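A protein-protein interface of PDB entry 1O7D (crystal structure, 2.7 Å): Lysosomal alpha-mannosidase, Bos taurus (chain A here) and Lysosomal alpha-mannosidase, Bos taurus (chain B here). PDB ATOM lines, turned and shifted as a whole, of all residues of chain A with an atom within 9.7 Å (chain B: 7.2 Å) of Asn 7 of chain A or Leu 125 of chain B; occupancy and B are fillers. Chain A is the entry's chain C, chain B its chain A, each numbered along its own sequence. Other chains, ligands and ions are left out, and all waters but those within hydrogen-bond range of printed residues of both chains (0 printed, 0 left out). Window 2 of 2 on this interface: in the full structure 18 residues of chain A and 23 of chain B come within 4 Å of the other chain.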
ATOM      1  N   ASP A   2       3.928  -0.307 -12.682  1.00  0.00           N
ATOM      2  CA  ASP A   2       4.157  -1.466 -11.808  1.00  0.00           C
ATOM      3  C   ASP A   2       5.605  -1.771 -11.394  1.00  0.00           C
ATOM      4  O   ASP A   2       6.476  -2.033 -12.237  1.00  0.00           O
ATOM      5  CB  ASP A   2       3.559  -2.723 -12.447  1.00  0.00           C
ATOM      6  CG  ASP A   2       3.346  -3.854 -11.435  1.00  0.00           C
ATOM      7  OD1 ASP A   2       3.770  -3.689 -10.258  1.00  0.00           O
ATOM      8  OD2 ASP A   2       2.754  -4.899 -11.818  1.00  0.00           O
ATOM      9  N   SER A   3       5.836  -1.775 -10.082  1.00  0.00           N
ATOM     10  CA  SER A   3       7.152  -2.052  -9.527  1.00  0.00           C
ATOM     11  C   SER A   3       7.399  -3.541  -9.342  1.00  0.00           C
ATOM     12  O   SER A   3       8.516  -3.934  -9.057  1.00  0.00           O
ATOM     13  CB  SER A   3       7.314  -1.356  -8.174  1.00  0.00           C
ATOM     14  OG  SER A   3       6.435  -1.898  -7.196  1.00  0.00           O
ATOM     15  N   ALA A   4       6.359  -4.359  -9.506  1.00  0.00           N
ATOM     16  CA  ALA A   4       6.454  -5.819  -9.330  1.00  0.00           C
ATOM     17  C   ALA A   4       7.450  -6.491 -10.273  1.00  0.00           C
ATOM     18  O   ALA A   4       8.290  -7.288  -9.844  1.00  0.00           O
ATOM     19  CB  ALA A   4       5.074  -6.466  -9.489  1.00  0.00           C
ATOM     20  N   PRO A   5       7.360  -6.183 -11.578  1.00  0.00           N
ATOM     21  CA  PRO A   5       8.276  -6.779 -12.551  1.00  0.00           C
ATOM     22  C   PRO A   5       9.764  -6.567 -12.255  1.00  0.00           C
ATOM     23  O   PRO A   5      10.567  -7.476 -12.419  1.00  0.00           O
ATOM     24  CB  PRO A   5       7.827  -6.156 -13.870  1.00  0.00           C
ATOM     25  CG  PRO A   5       7.119  -4.880 -13.429  1.00  0.00           C
ATOM     26  CD  PRO A   5       6.367  -5.326 -12.248  1.00  0.00           C
ATOM     27  N   LEU A   6      10.139  -5.386 -11.803  1.00  0.00           N
ATOM     28  CA  LEU A   6      11.535  -5.162 -11.519  1.00  0.00           C
ATOM     29  C   LEU A   6      11.982  -5.853 -10.229  1.00  0.00           C
ATOM     30  O   LEU A   6      13.116  -6.331 -10.149  1.00  0.00           O
ATOM     31  CB  LEU A   6      11.814  -3.669 -11.439  1.00  0.00           C
ATOM     32  CG  LEU A   6      13.269  -3.299 -11.182  1.00  0.00           C
ATOM     33  CD1 LEU A   6      14.114  -3.715 -12.370  1.00  0.00           C
ATOM     34  CD2 LEU A   6      13.381  -1.809 -10.942  1.00  0.00           C
ATOM     35  N   ASN A   7      11.105  -5.909  -9.223  1.00  0.00           N
ATOM     36  CA  ASN A   7      11.427  -6.551  -7.933  1.00  0.00           C
ATOM     37  C   ASN A   7      11.690  -8.033  -8.132  1.00  0.00           C
ATOM     38  O   ASN A   7      12.514  -8.643  -7.452  1.00  0.00           O
ATOM     39  CB  ASN A   7      10.270  -6.410  -6.944  1.00  0.00           C
ATOM     40  CG  ASN A   7      10.596  -6.988  -5.569  1.00  0.00           C
ATOM     41  OD1 ASN A   7      11.325  -6.385  -4.770  1.00  0.00           O
ATOM     42  ND2 ASN A   7      10.060  -8.164  -5.294  1.00  0.00           N
ATOM     43  N   GLU A   8      10.955  -8.597  -9.077  1.00  0.00           N
ATOM     44  CA  GLU A   8      11.049  -9.998  -9.444  1.00  0.00           C
ATOM     45  C   GLU A   8      12.352 -10.313 -10.194  1.00  0.00           C
ATOM     46  O   GLU A   8      13.008 -11.303  -9.902  1.00  0.00           O
ATOM     47  CB  GLU A   8       9.859 -10.343 -10.321  1.00  0.00           C
ATOM     48  CG  GLU A   8       9.576 -11.803 -10.395  1.00  0.00           C
ATOM     49  CD  GLU A   8       8.350 -12.095 -11.218  1.00  0.00           C
ATOM     50  OE1 GLU A   8       7.288 -11.513 -10.895  1.00  0.00           O
ATOM     51  OE2 GLU A   8       8.447 -12.904 -12.175  1.00  0.00           O
ATOM     52  N   ALA A   9      12.710  -9.471 -11.168  1.00  0.00           N
ATOM     53  CA  ALA A   9      13.924  -9.654 -11.955  1.00  0.00           C
ATOM     54  C   ALA A   9      15.175  -9.492 -11.077  1.00  0.00           C
ATOM     55  O   ALA A   9      16.182 -10.184 -11.265  1.00  0.00           O
ATOM     56  CB  ALA A   9      13.947  -8.665 -13.124  1.00  0.00           C
ATOM     57  N   MET A  10      15.112  -8.574 -10.120  1.00  0.00           N
ATOM     58  CA  MET A  10      16.220  -8.373  -9.194  1.00  0.00           C
ATOM     59  C   MET A  10      16.378  -9.627  -8.329  1.00  0.00           C
ATOM     60  O   MET A  10      17.466  -9.957  -7.872  1.00  0.00           O
ATOM     61  CB  MET A  10      15.946  -7.171  -8.302  1.00  0.00           C
ATOM     62  CG  MET A  10      16.397  -5.871  -8.876  1.00  0.00           C
ATOM     63  SD  MET A  10      18.151  -5.886  -8.976  1.00  0.00           S
ATOM     64  CE  MET A  10      18.601  -6.199  -7.203  1.00  0.00           C
ATOM     65  N   ALA A  11      15.276 -10.323  -8.088  1.00  0.00           N
ATOM     66  CA  ALA A  11      15.332 -11.541  -7.303  1.00  0.00           C
ATOM     67  C   ALA A  11      16.027 -12.618  -8.140  1.00  0.00           C
ATOM     68  O   ALA A  11      16.951 -13.283  -7.674  1.00  0.00           O
ATOM     69  CB  ALA A  11      13.913 -11.987  -6.926  1.00  0.00           C
ATOM     70  N   VAL A  12      15.581 -12.772  -9.384  1.00  0.00           N
ATOM     71  CA  VAL A  12      16.147 -13.757 -10.287  1.00  0.00           C
ATOM     72  C   VAL A  12      17.651 -13.578 -10.381  1.00  0.00           C
ATOM     73  O   VAL A  12      18.417 -14.529 -10.211  1.00  0.00           O
ATOM     74  CB  VAL A  12      15.557 -13.627 -11.709  1.00  0.00           C
ATOM     75  CG1 VAL A  12      16.211 -14.634 -12.640  1.00  0.00           C
ATOM     76  CG2 VAL A  12      14.060 -13.855 -11.676  1.00  0.00           C
ATOM     77  N   LEU A  13      18.083 -12.354 -10.644  1.00  0.00           N
ATOM     78  CA  LEU A  13      19.502 -12.116 -10.776  1.00  0.00           C
ATOM     79  C   LEU A  13      20.274 -12.446  -9.505  1.00  0.00           C
ATOM     80  O   LEU A  13      21.505 -12.506  -9.504  1.00  0.00           O
ATOM     81  CB  LEU A  13      19.749 -10.671 -11.188  1.00  0.00           C
ATOM     82  CG  LEU A  13      19.202 -10.264 -12.560  1.00  0.00           C
ATOM     83  CD1 LEU A  13      19.606  -8.865 -12.737  1.00  0.00           C
ATOM     84  CD2 LEU A  13      19.759 -11.064 -13.708  1.00  0.00           C
ATOM     85  N   GLN A  14      19.564 -12.679  -8.417  1.00  0.00           N
ATOM     86  CA  GLN A  14      20.242 -12.989  -7.182  1.00  0.00           C
ATOM     87  C   GLN A  14      20.634 -14.439  -7.140  1.00  0.00           C
ATOM     88  O   GLN A  14      21.331 -14.873  -6.230  1.00  0.00           O
ATOM     89  CB  GLN A  14      19.352 -12.634  -6.004  1.00  0.00           C
ATOM     90  CG  GLN A  14      19.085 -11.157  -5.938  1.00  0.00           C
ATOM     91  CD  GLN A  14      20.361 -10.370  -5.817  1.00  0.00           C
ATOM     92  OE1 GLN A  14      21.403 -10.776  -6.315  1.00  0.00           O
ATOM     93  NE2 GLN A  14      20.290  -9.239  -5.160  1.00  0.00           N
ATOM     94  N   GLN A  34      15.350  -9.651 -18.715  1.00  0.00           N
ATOM     95  CA  GLN A  34      14.312  -9.582 -17.673  1.00  0.00           C
ATOM     96  C   GLN A  34      14.414  -8.271 -16.901  1.00  0.00           C
ATOM     97  O   GLN A  34      13.400  -7.722 -16.475  1.00  0.00           O
ATOM     98  CB  GLN A  34      14.422 -10.749 -16.670  1.00  0.00           C
ATOM     99  CG  GLN A  34      13.886 -12.091 -17.159  1.00  0.00           C
ATOM    100  CD  GLN A  34      14.085 -13.218 -16.131  1.00  0.00           C
ATOM    101  OE1 GLN A  34      13.458 -13.226 -15.057  1.00  0.00           O
ATOM    102  NE2 GLN A  34      14.968 -14.172 -16.456  1.00  0.00           N
ATOM    103  N   LEU A  35      15.640  -7.789 -16.708  1.00  0.00           N
ATOM    104  CA  LEU A  35      15.873  -6.532 -16.005  1.00  0.00           C
ATOM    105  C   LEU A  35      15.444  -5.326 -16.817  1.00  0.00           C
ATOM    106  O   LEU A  35      14.887  -4.381 -16.283  1.00  0.00           O
ATOM    107  CB  LEU A  35      17.346  -6.357 -15.697  1.00  0.00           C
ATOM    108  CG  LEU A  35      17.908  -6.999 -14.450  1.00  0.00           C
ATOM    109  CD1 LEU A  35      19.219  -6.296 -14.149  1.00  0.00           C
ATOM    110  CD2 LEU A  35      16.943  -6.858 -13.287  1.00  0.00           C
ATOM    111  N   GLU A  37      13.164  -5.183 -19.087  1.00  0.00           N
ATOM    112  CA  GLU A  37      11.716  -5.147 -19.098  1.00  0.00           C
ATOM    113  C   GLU A  37      11.058  -4.795 -17.761  1.00  0.00           C
ATOM    114  O   GLU A  37       9.857  -4.524 -17.710  1.00  0.00           O
ATOM    115  CB  GLU A  37      11.185  -6.467 -19.641  1.00  0.00           C
ATOM    116  CG  GLU A  37      11.345  -6.569 -21.154  1.00  0.00           C
ATOM    117  CD  GLU A  37      10.933  -7.925 -21.691  1.00  0.00           C
ATOM    118  OE1 GLU A  37      11.479  -8.932 -21.172  1.00  0.00           O
ATOM    119  OE2 GLU A  37      10.080  -7.984 -22.620  1.00  0.00           O
ATOM    120  N   GLY A  38      11.842  -4.782 -16.689  1.00  0.00           N
ATOM    121  CA  GLY A  38      11.303  -4.422 -15.391  1.00  0.00           C
ATOM    122  C   GLY A  38      11.434  -2.923 -15.148  1.00  0.00           C
ATOM    123  O   GLY A  38      10.730  -2.342 -14.315  1.00  0.00           O
ATOM    124  N   TRP A  39      12.344  -2.296 -15.890  1.00  0.00           N
ATOM    125  CA  TRP A  39      12.601  -0.865 -15.778  1.00  0.00           C
ATOM    126  C   TRP A  39      11.502   0.007 -16.380  1.00  0.00           C
ATOM    127  O   TRP A  39      11.325   1.148 -15.976  1.00  0.00           O
ATOM    128  CB  TRP A  39      13.931  -0.511 -16.454  1.00  0.00           C
ATOM    129  CG  TRP A  39      15.191  -0.715 -15.624  1.00  0.00           C
ATOM    130  CD1 TRP A  39      15.688  -1.896 -15.140  1.00  0.00           C
ATOM    131  CD2 TRP A  39      16.146   0.294 -15.265  1.00  0.00           C
ATOM    132  NE1 TRP A  39      16.892  -1.684 -14.510  1.00  0.00           N
ATOM    133  CE2 TRP A  39      17.197  -0.351 -14.570  1.00  0.00           C
ATOM    134  CE3 TRP A  39      16.211   1.680 -15.460  1.00  0.00           C
ATOM    135  CZ2 TRP A  39      18.302   0.342 -14.076  1.00  0.00           C
ATOM    136  CZ3 TRP A  39      17.304   2.365 -14.968  1.00  0.00           C
ATOM    137  CH2 TRP A  39      18.338   1.695 -14.281  1.00  0.00           C
ATOM    138  N   PRO A  41       7.873  -0.526 -16.552  1.00  0.00           N
ATOM    139  CA  PRO A  41       6.754  -0.303 -15.647  1.00  0.00           C
ATOM    140  C   PRO A  41       7.116   0.571 -14.472  1.00  0.00           C
ATOM    141  O   PRO A  41       6.265   1.295 -13.974  1.00  0.00           O
ATOM    142  CB  PRO A  41       6.370  -1.717 -15.231  1.00  0.00           C
ATOM    143  CG  PRO A  41       6.714  -2.518 -16.420  1.00  0.00           C
ATOM    144  CD  PRO A  41       8.069  -1.966 -16.774  1.00  0.00           C
ATOM    145  N   CYS A  42       8.378   0.520 -14.040  1.00  0.00           N
ATOM    146  CA  CYS A  42       8.804   1.324 -12.890  1.00  0.00           C
ATOM    147  C   CYS A  42       8.879   2.812 -13.161  1.00  0.00           C
ATOM    148  O   CYS A  42       8.493   3.618 -12.304  1.00  0.00           O
ATOM    149  CB  CYS A  42      10.154   0.867 -12.319  1.00  0.00           C
ATOM    150  SG  CYS A  42       9.993   0.000 -10.718  1.00  0.00           S
ATOM    151  N   ILE B  72      11.384 -20.969  -4.898  1.00  0.00           N
ATOM    152  CA  ILE B  72      10.040 -20.437  -4.987  1.00  0.00           C
ATOM    153  C   ILE B  72       9.672 -19.881  -6.356  1.00  0.00           C
ATOM    154  O   ILE B  72       8.506 -19.913  -6.748  1.00  0.00           O
ATOM    155  CB  ILE B  72       9.815 -19.358  -3.929  1.00  0.00           C
ATOM    156  CG1 ILE B  72      10.096 -19.939  -2.547  1.00  0.00           C
ATOM    157  CG2 ILE B  72       8.371 -18.869  -3.982  1.00  0.00           C
ATOM    158  CD1 ILE B  72       9.261 -21.145  -2.220  1.00  0.00           C
ATOM    159  N   GLY B 104      13.094 -21.040   0.927  1.00  0.00           N
ATOM    160  CA  GLY B 104      12.014 -20.069   0.906  1.00  0.00           C
ATOM    161  C   GLY B 104      12.258 -18.821   0.078  1.00  0.00           C
ATOM    162  O   GLY B 104      11.355 -18.003  -0.120  1.00  0.00           O
ATOM    163  N   GLY B 105      13.486 -18.653  -0.395  1.00  0.00           N
ATOM    164  CA  GLY B 105      13.782 -17.489  -1.203  1.00  0.00           C
ATOM    165  C   GLY B 105      13.216 -17.661  -2.596  1.00  0.00           C
ATOM    166  O   GLY B 105      12.809 -18.756  -2.981  1.00  0.00           O
ATOM    167  N   TRP B 106      13.181 -16.575  -3.356  1.00  0.00           N
ATOM    168  CA  TRP B 106      12.670 -16.626  -4.714  1.00  0.00           C
ATOM    169  C   TRP B 106      13.601 -17.557  -5.451  1.00  0.00           C
ATOM    170  O   TRP B 106      13.181 -18.277  -6.350  1.00  0.00           O
ATOM    171  CB  TRP B 106      12.684 -15.229  -5.345  1.00  0.00           C
ATOM    172  CG  TRP B 106      12.036 -15.160  -6.689  1.00  0.00           C
ATOM    173  CD1 TRP B 106      12.656 -14.950  -7.866  1.00  0.00           C
ATOM    174  CD2 TRP B 106      10.638 -15.281  -6.988  1.00  0.00           C
ATOM    175  NE1 TRP B 106      11.746 -14.927  -8.892  1.00  0.00           N
ATOM    176  CE2 TRP B 106      10.496 -15.129  -8.379  1.00  0.00           C
ATOM    177  CE3 TRP B 106       9.492 -15.507  -6.215  1.00  0.00           C
ATOM    178  CZ2 TRP B 106       9.260 -15.188  -9.020  1.00  0.00           C
ATOM    179  CZ3 TRP B 106       8.257 -15.569  -6.857  1.00  0.00           C
ATOM    180  CH2 TRP B 106       8.156 -15.411  -8.247  1.00  0.00           C
ATOM    181  N   ILE B 119      19.602  -9.282  -1.227  1.00  0.00           N
ATOM    182  CA  ILE B 119      19.363 -10.632  -0.747  1.00  0.00           C
ATOM    183  C   ILE B 119      18.055 -10.651   0.039  1.00  0.00           C
ATOM    184  O   ILE B 119      17.308 -11.618   0.009  1.00  0.00           O
ATOM    185  CB  ILE B 119      20.509 -11.084   0.178  1.00  0.00           C
ATOM    186  CG1 ILE B 119      21.787 -11.244  -0.639  1.00  0.00           C
ATOM    187  CG2 ILE B 119      20.152 -12.381   0.887  1.00  0.00           C
ATOM    188  CD1 ILE B 119      23.036 -11.372   0.216  1.00  0.00           C
ATOM    189  N   ILE B 120      17.782  -9.571   0.749  1.00  0.00           N
ATOM    190  CA  ILE B 120      16.564  -9.490   1.533  1.00  0.00           C
ATOM    191  C   ILE B 120      15.322  -9.366   0.647  1.00  0.00           C
ATOM    192  O   ILE B 120      14.336 -10.081   0.846  1.00  0.00           O
ATOM    193  CB  ILE B 120      16.638  -8.309   2.510  1.00  0.00           C
ATOM    194  CG1 ILE B 120      17.879  -8.464   3.392  1.00  0.00           C
ATOM    195  CG2 ILE B 120      15.377  -8.247   3.363  1.00  0.00           C
ATOM    196  CD1 ILE B 120      18.096  -7.299   4.350  1.00  0.00           C
ATOM    197  N   ASP B 121      15.353  -8.460  -0.327  1.00  0.00           N
ATOM    198  CA  ASP B 121      14.202  -8.324  -1.212  1.00  0.00           C
ATOM    199  C   ASP B 121      13.880  -9.688  -1.824  1.00  0.00           C
ATOM    200  O   ASP B 121      12.717 -10.096  -1.889  1.00  0.00           O
ATOM    201  CB  ASP B 121      14.472  -7.302  -2.326  1.00  0.00           C
ATOM    202  CG  ASP B 121      14.634  -5.874  -1.788  1.00  0.00           C
ATOM    203  OD1 ASP B 121      13.776  -5.425  -1.005  1.00  0.00           O
ATOM    204  OD2 ASP B 121      15.609  -5.177  -2.147  1.00  0.00           O
ATOM    205  N   GLN B 122      14.929 -10.384  -2.255  1.00  0.00           N
ATOM    206  CA  GLN B 122      14.820 -11.696  -2.863  1.00  0.00           C
ATOM    207  C   GLN B 122      14.163 -12.681  -1.891  1.00  0.00           C
ATOM    208  O   GLN B 122      13.203 -13.364  -2.246  1.00  0.00           O
ATOM    209  CB  GLN B 122      16.223 -12.174  -3.271  1.00  0.00           C
ATOM    210  CG  GLN B 122      16.284 -13.526  -3.956  1.00  0.00           C
ATOM    211  CD  GLN B 122      16.346 -14.700  -2.991  1.00  0.00           C
ATOM    212  OE1 GLN B 122      15.651 -15.688  -3.168  1.00  0.00           O
ATOM    213  NE2 GLN B 122      17.195 -14.604  -1.985  1.00  0.00           N
ATOM    214  N   MET B 123      14.657 -12.737  -0.661  1.00  0.00           N
ATOM    215  CA  MET B 123      14.093 -13.657   0.312  1.00  0.00           C
ATOM    216  C   MET B 123      12.647 -13.312   0.658  1.00  0.00           C
ATOM    217  O   MET B 123      11.767 -14.167   0.589  1.00  0.00           O
ATOM    218  CB  MET B 123      14.944 -13.661   1.575  1.00  0.00           C
ATOM    219  CG  MET B 123      15.058 -15.036   2.210  1.00  0.00           C
ATOM    220  SD  MET B 123      16.046 -16.158   1.211  1.00  0.00           S
ATOM    221  CE  MET B 123      17.566 -15.431   1.452  1.00  0.00           C
ATOM    222  N   THR B 124      12.409 -12.058   1.031  1.00  0.00           N
ATOM    223  CA  THR B 124      11.073 -11.582   1.372  1.00  0.00           C
ATOM    224  C   THR B 124      10.089 -11.984   0.290  1.00  0.00           C
ATOM    225  O   THR B 124       8.949 -12.311   0.568  1.00  0.00           O
ATOM    226  CB  THR B 124      11.030 -10.042   1.462  1.00  0.00           C
ATOM    227  OG1 THR B 124      11.783  -9.592   2.594  1.00  0.00           O
ATOM    228  CG2 THR B 124       9.603  -9.554   1.568  1.00  0.00           C
ATOM    229  N   LEU B 125      10.540 -11.945  -0.955  1.00  0.00           N
ATOM    230  CA  LEU B 125       9.684 -12.270  -2.081  1.00  0.00           C
ATOM    231  C   LEU B 125       9.244 -13.734  -2.078  1.00  0.00           C
ATOM    232  O   LEU B 125       8.079 -14.044  -2.362  1.00  0.00           O
ATOM    233  CB  LEU B 125      10.399 -11.916  -3.389  1.00  0.00           C
ATOM    234  CG  LEU B 125       9.638 -12.159  -4.694  1.00  0.00           C
ATOM    235  CD1 LEU B 125       8.256 -11.552  -4.598  1.00  0.00           C
ATOM    236  CD2 LEU B 125      10.420 -11.572  -5.866  1.00  0.00           C
ATOM    237  N   GLY B 126      10.163 -14.636  -1.753  1.00  0.00           N
ATOM    238  CA  GLY B 126       9.808 -16.039  -1.738  1.00  0.00           C
ATOM    239  C   GLY B 126       8.938 -16.329  -0.533  1.00  0.00           C
ATOM    240  O   GLY B 126       7.841 -16.892  -0.650  1.00  0.00           O
ATOM    241  N   LEU B 127       9.448 -15.932   0.630  1.00  0.00           N
ATOM    242  CA  LEU B 127       8.762 -16.117   1.898  1.00  0.00           C
ATOM    243  C   LEU B 127       7.391 -15.451   1.872  1.00  0.00           C
ATOM    244  O   LEU B 127       6.462 -15.875   2.560  1.00  0.00           O
ATOM    245  CB  LEU B 127       9.629 -15.555   3.026  1.00  0.00           C
ATOM    246  CG  LEU B 127      10.995 -16.255   3.101  1.00  0.00           C
ATOM    247  CD1 LEU B 127      11.836 -15.708   4.229  1.00  0.00           C
ATOM    248  CD2 LEU B 127      10.790 -17.729   3.284  1.00  0.00           C
ATOM    249  N   ARG B 128       7.257 -14.415   1.059  1.00  0.00           N
ATOM    250  CA  ARG B 128       5.989 -13.720   0.949  1.00  0.00           C
ATOM    251  C   ARG B 128       4.973 -14.659   0.286  1.00  0.00           C
ATOM    252  O   ARG B 128       3.849 -14.825   0.782  1.00  0.00           O
ATOM    253  CB  ARG B 128       6.165 -12.439   0.126  1.00  0.00           C
ATOM    254  CG  ARG B 128       5.163 -11.313   0.432  1.00  0.00           C
ATOM    255  CD  ARG B 128       4.116 -11.196  -0.655  1.00  0.00           C
ATOM    256  NE  ARG B 128       3.076 -10.239  -0.303  1.00  0.00           N
ATOM    257  CZ  ARG B 128       3.230  -8.919  -0.315  1.00  0.00           C
ATOM    258  NH1 ARG B 128       4.394  -8.400  -0.682  1.00  0.00           N
ATOM    259  NH2 ARG B 128       2.237  -8.117   0.082  1.00  0.00           N
ATOM    260  N   PHE B 129       5.372 -15.281  -0.824  1.00  0.00           N
ATOM    261  CA  PHE B 129       4.486 -16.201  -1.538  1.00  0.00           C
ATOM    262  C   PHE B 129       4.020 -17.339  -0.658  1.00  0.00           C
ATOM    263  O   PHE B 129       2.829 -17.626  -0.580  1.00  0.00           O
ATOM    264  CB  PHE B 129       5.168 -16.819  -2.761  1.00  0.00           C
ATOM    265  CG  PHE B 129       4.429 -18.012  -3.310  1.00  0.00           C
ATOM    266  CD1 PHE B 129       3.198 -17.867  -3.919  1.00  0.00           C
ATOM    267  CD2 PHE B 129       4.931 -19.290  -3.151  1.00  0.00           C
ATOM    268  CE1 PHE B 129       2.479 -18.978  -4.350  1.00  0.00           C
ATOM    269  CE2 PHE B 129       4.212 -20.398  -3.582  1.00  0.00           C
ATOM    270  CZ  PHE B 129       2.991 -20.241  -4.179  1.00  0.00           C
ATOM    271  N   LEU B 130       4.980 -18.010  -0.032  1.00  0.00           N
ATOM    272  CA  LEU B 130       4.688 -19.132   0.841  1.00  0.00           C
ATOM    273  C   LEU B 130       3.749 -18.662   1.933  1.00  0.00           C
ATOM    274  O   LEU B 130       2.702 -19.272   2.195  1.00  0.00           O
ATOM    275  CB  LEU B 130       5.969 -19.675   1.480  1.00  0.00           C
ATOM    276  CG  LEU B 130       6.994 -20.351   0.568  1.00  0.00           C
ATOM    277  CD1 LEU B 130       8.192 -20.836   1.377  1.00  0.00           C
ATOM    278  CD2 LEU B 130       6.343 -21.515  -0.138  1.00  0.00           C
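Of chain B, only Leu 125 comes within 4 Å of Asn 7 of chain A.
Leu 125 of chain B touches three residues of chain A.
No residue of chain A comes within 4 Å of Gly 126 of chain B.
Of the printed residues of chain A, Ile 119 of chain B touches Gln 14 (3.99 Å).
Printed residues of chain A within 4 Å of Gln 122 of chain B: Ala 11 and Gln 14.
Printed residues of chain B within 4 Å of Gln 14 of chain A: Ile 119 (3.99 Å) and Gln 122 (3.8 Å).
Printed residues of chain B within 4 Å of Glu 8 of chain A: Trp 106 (3.7 Å) and Leu 125 (3.96 Å).
The nearest residue of chain A that does not touch Leu 125 of chain B is Ala 9 of chain A (6.1 Å).
The nearest printed residue of chain A that does not touch Gln 122 of chain B is Met 10 of chain A (5.3 Å).
The backbone NH (N) of Trp 106 of chain B sits at hydrogen-bond distance from the side-chain amide oxygen (OE1) of Gln 122 of chain B, at 2.6 Å.
The side-chain amide nitrogen (NE2) of Gln 122 of chain B lies close to the side-chain sulfur (SD) of Met 123 of chain B (3.7 Å).
Asn 7 of chain A touches Leu 125 of chain B.
CZ2 of Trp 106 of chain B touches CG of Glu 8 of chain A (3.7 Å).
Leu 125 of chain B touches Glu 8 of chain A (CD2 to CA, 3.96 Å).
Ala 11 of chain A touches Trp 106 of chain B (CB to CD1, 3.4 Å).
O of Ala 11 of chain A touches CG of Gln 122 of chain B, 3.8 Å away.
Leu 125 of chain B touches Ala 11 of chain A (CD2 to CB, 3.7 Å).
CG2 of Val 12 of chain A touches NE1 of Trp 106 of chain B (3.8 Å).
Ile 119 of chain B touches Gln 14 of chain A (N to NE2, 3.99 Å).
Gln 122 of chain B touches Gln 14 of chain A.
Of the 16 printed residues of chain B, 4 touch a printed residue of chain A.
Hydrophobic or aromatic side chains of chain B that line the printed part of chain A: Trp 106 and Leu 125.
Along chain B the printed residues that touch a printed residue of chain A span positions 106 to 125.
Of the 20 printed residues of chain A, 5 touch a printed residue of chain B.
Hydrophobic or aromatic side chains of chain A that line the printed part of chain B: Ala 11 and Val 12.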
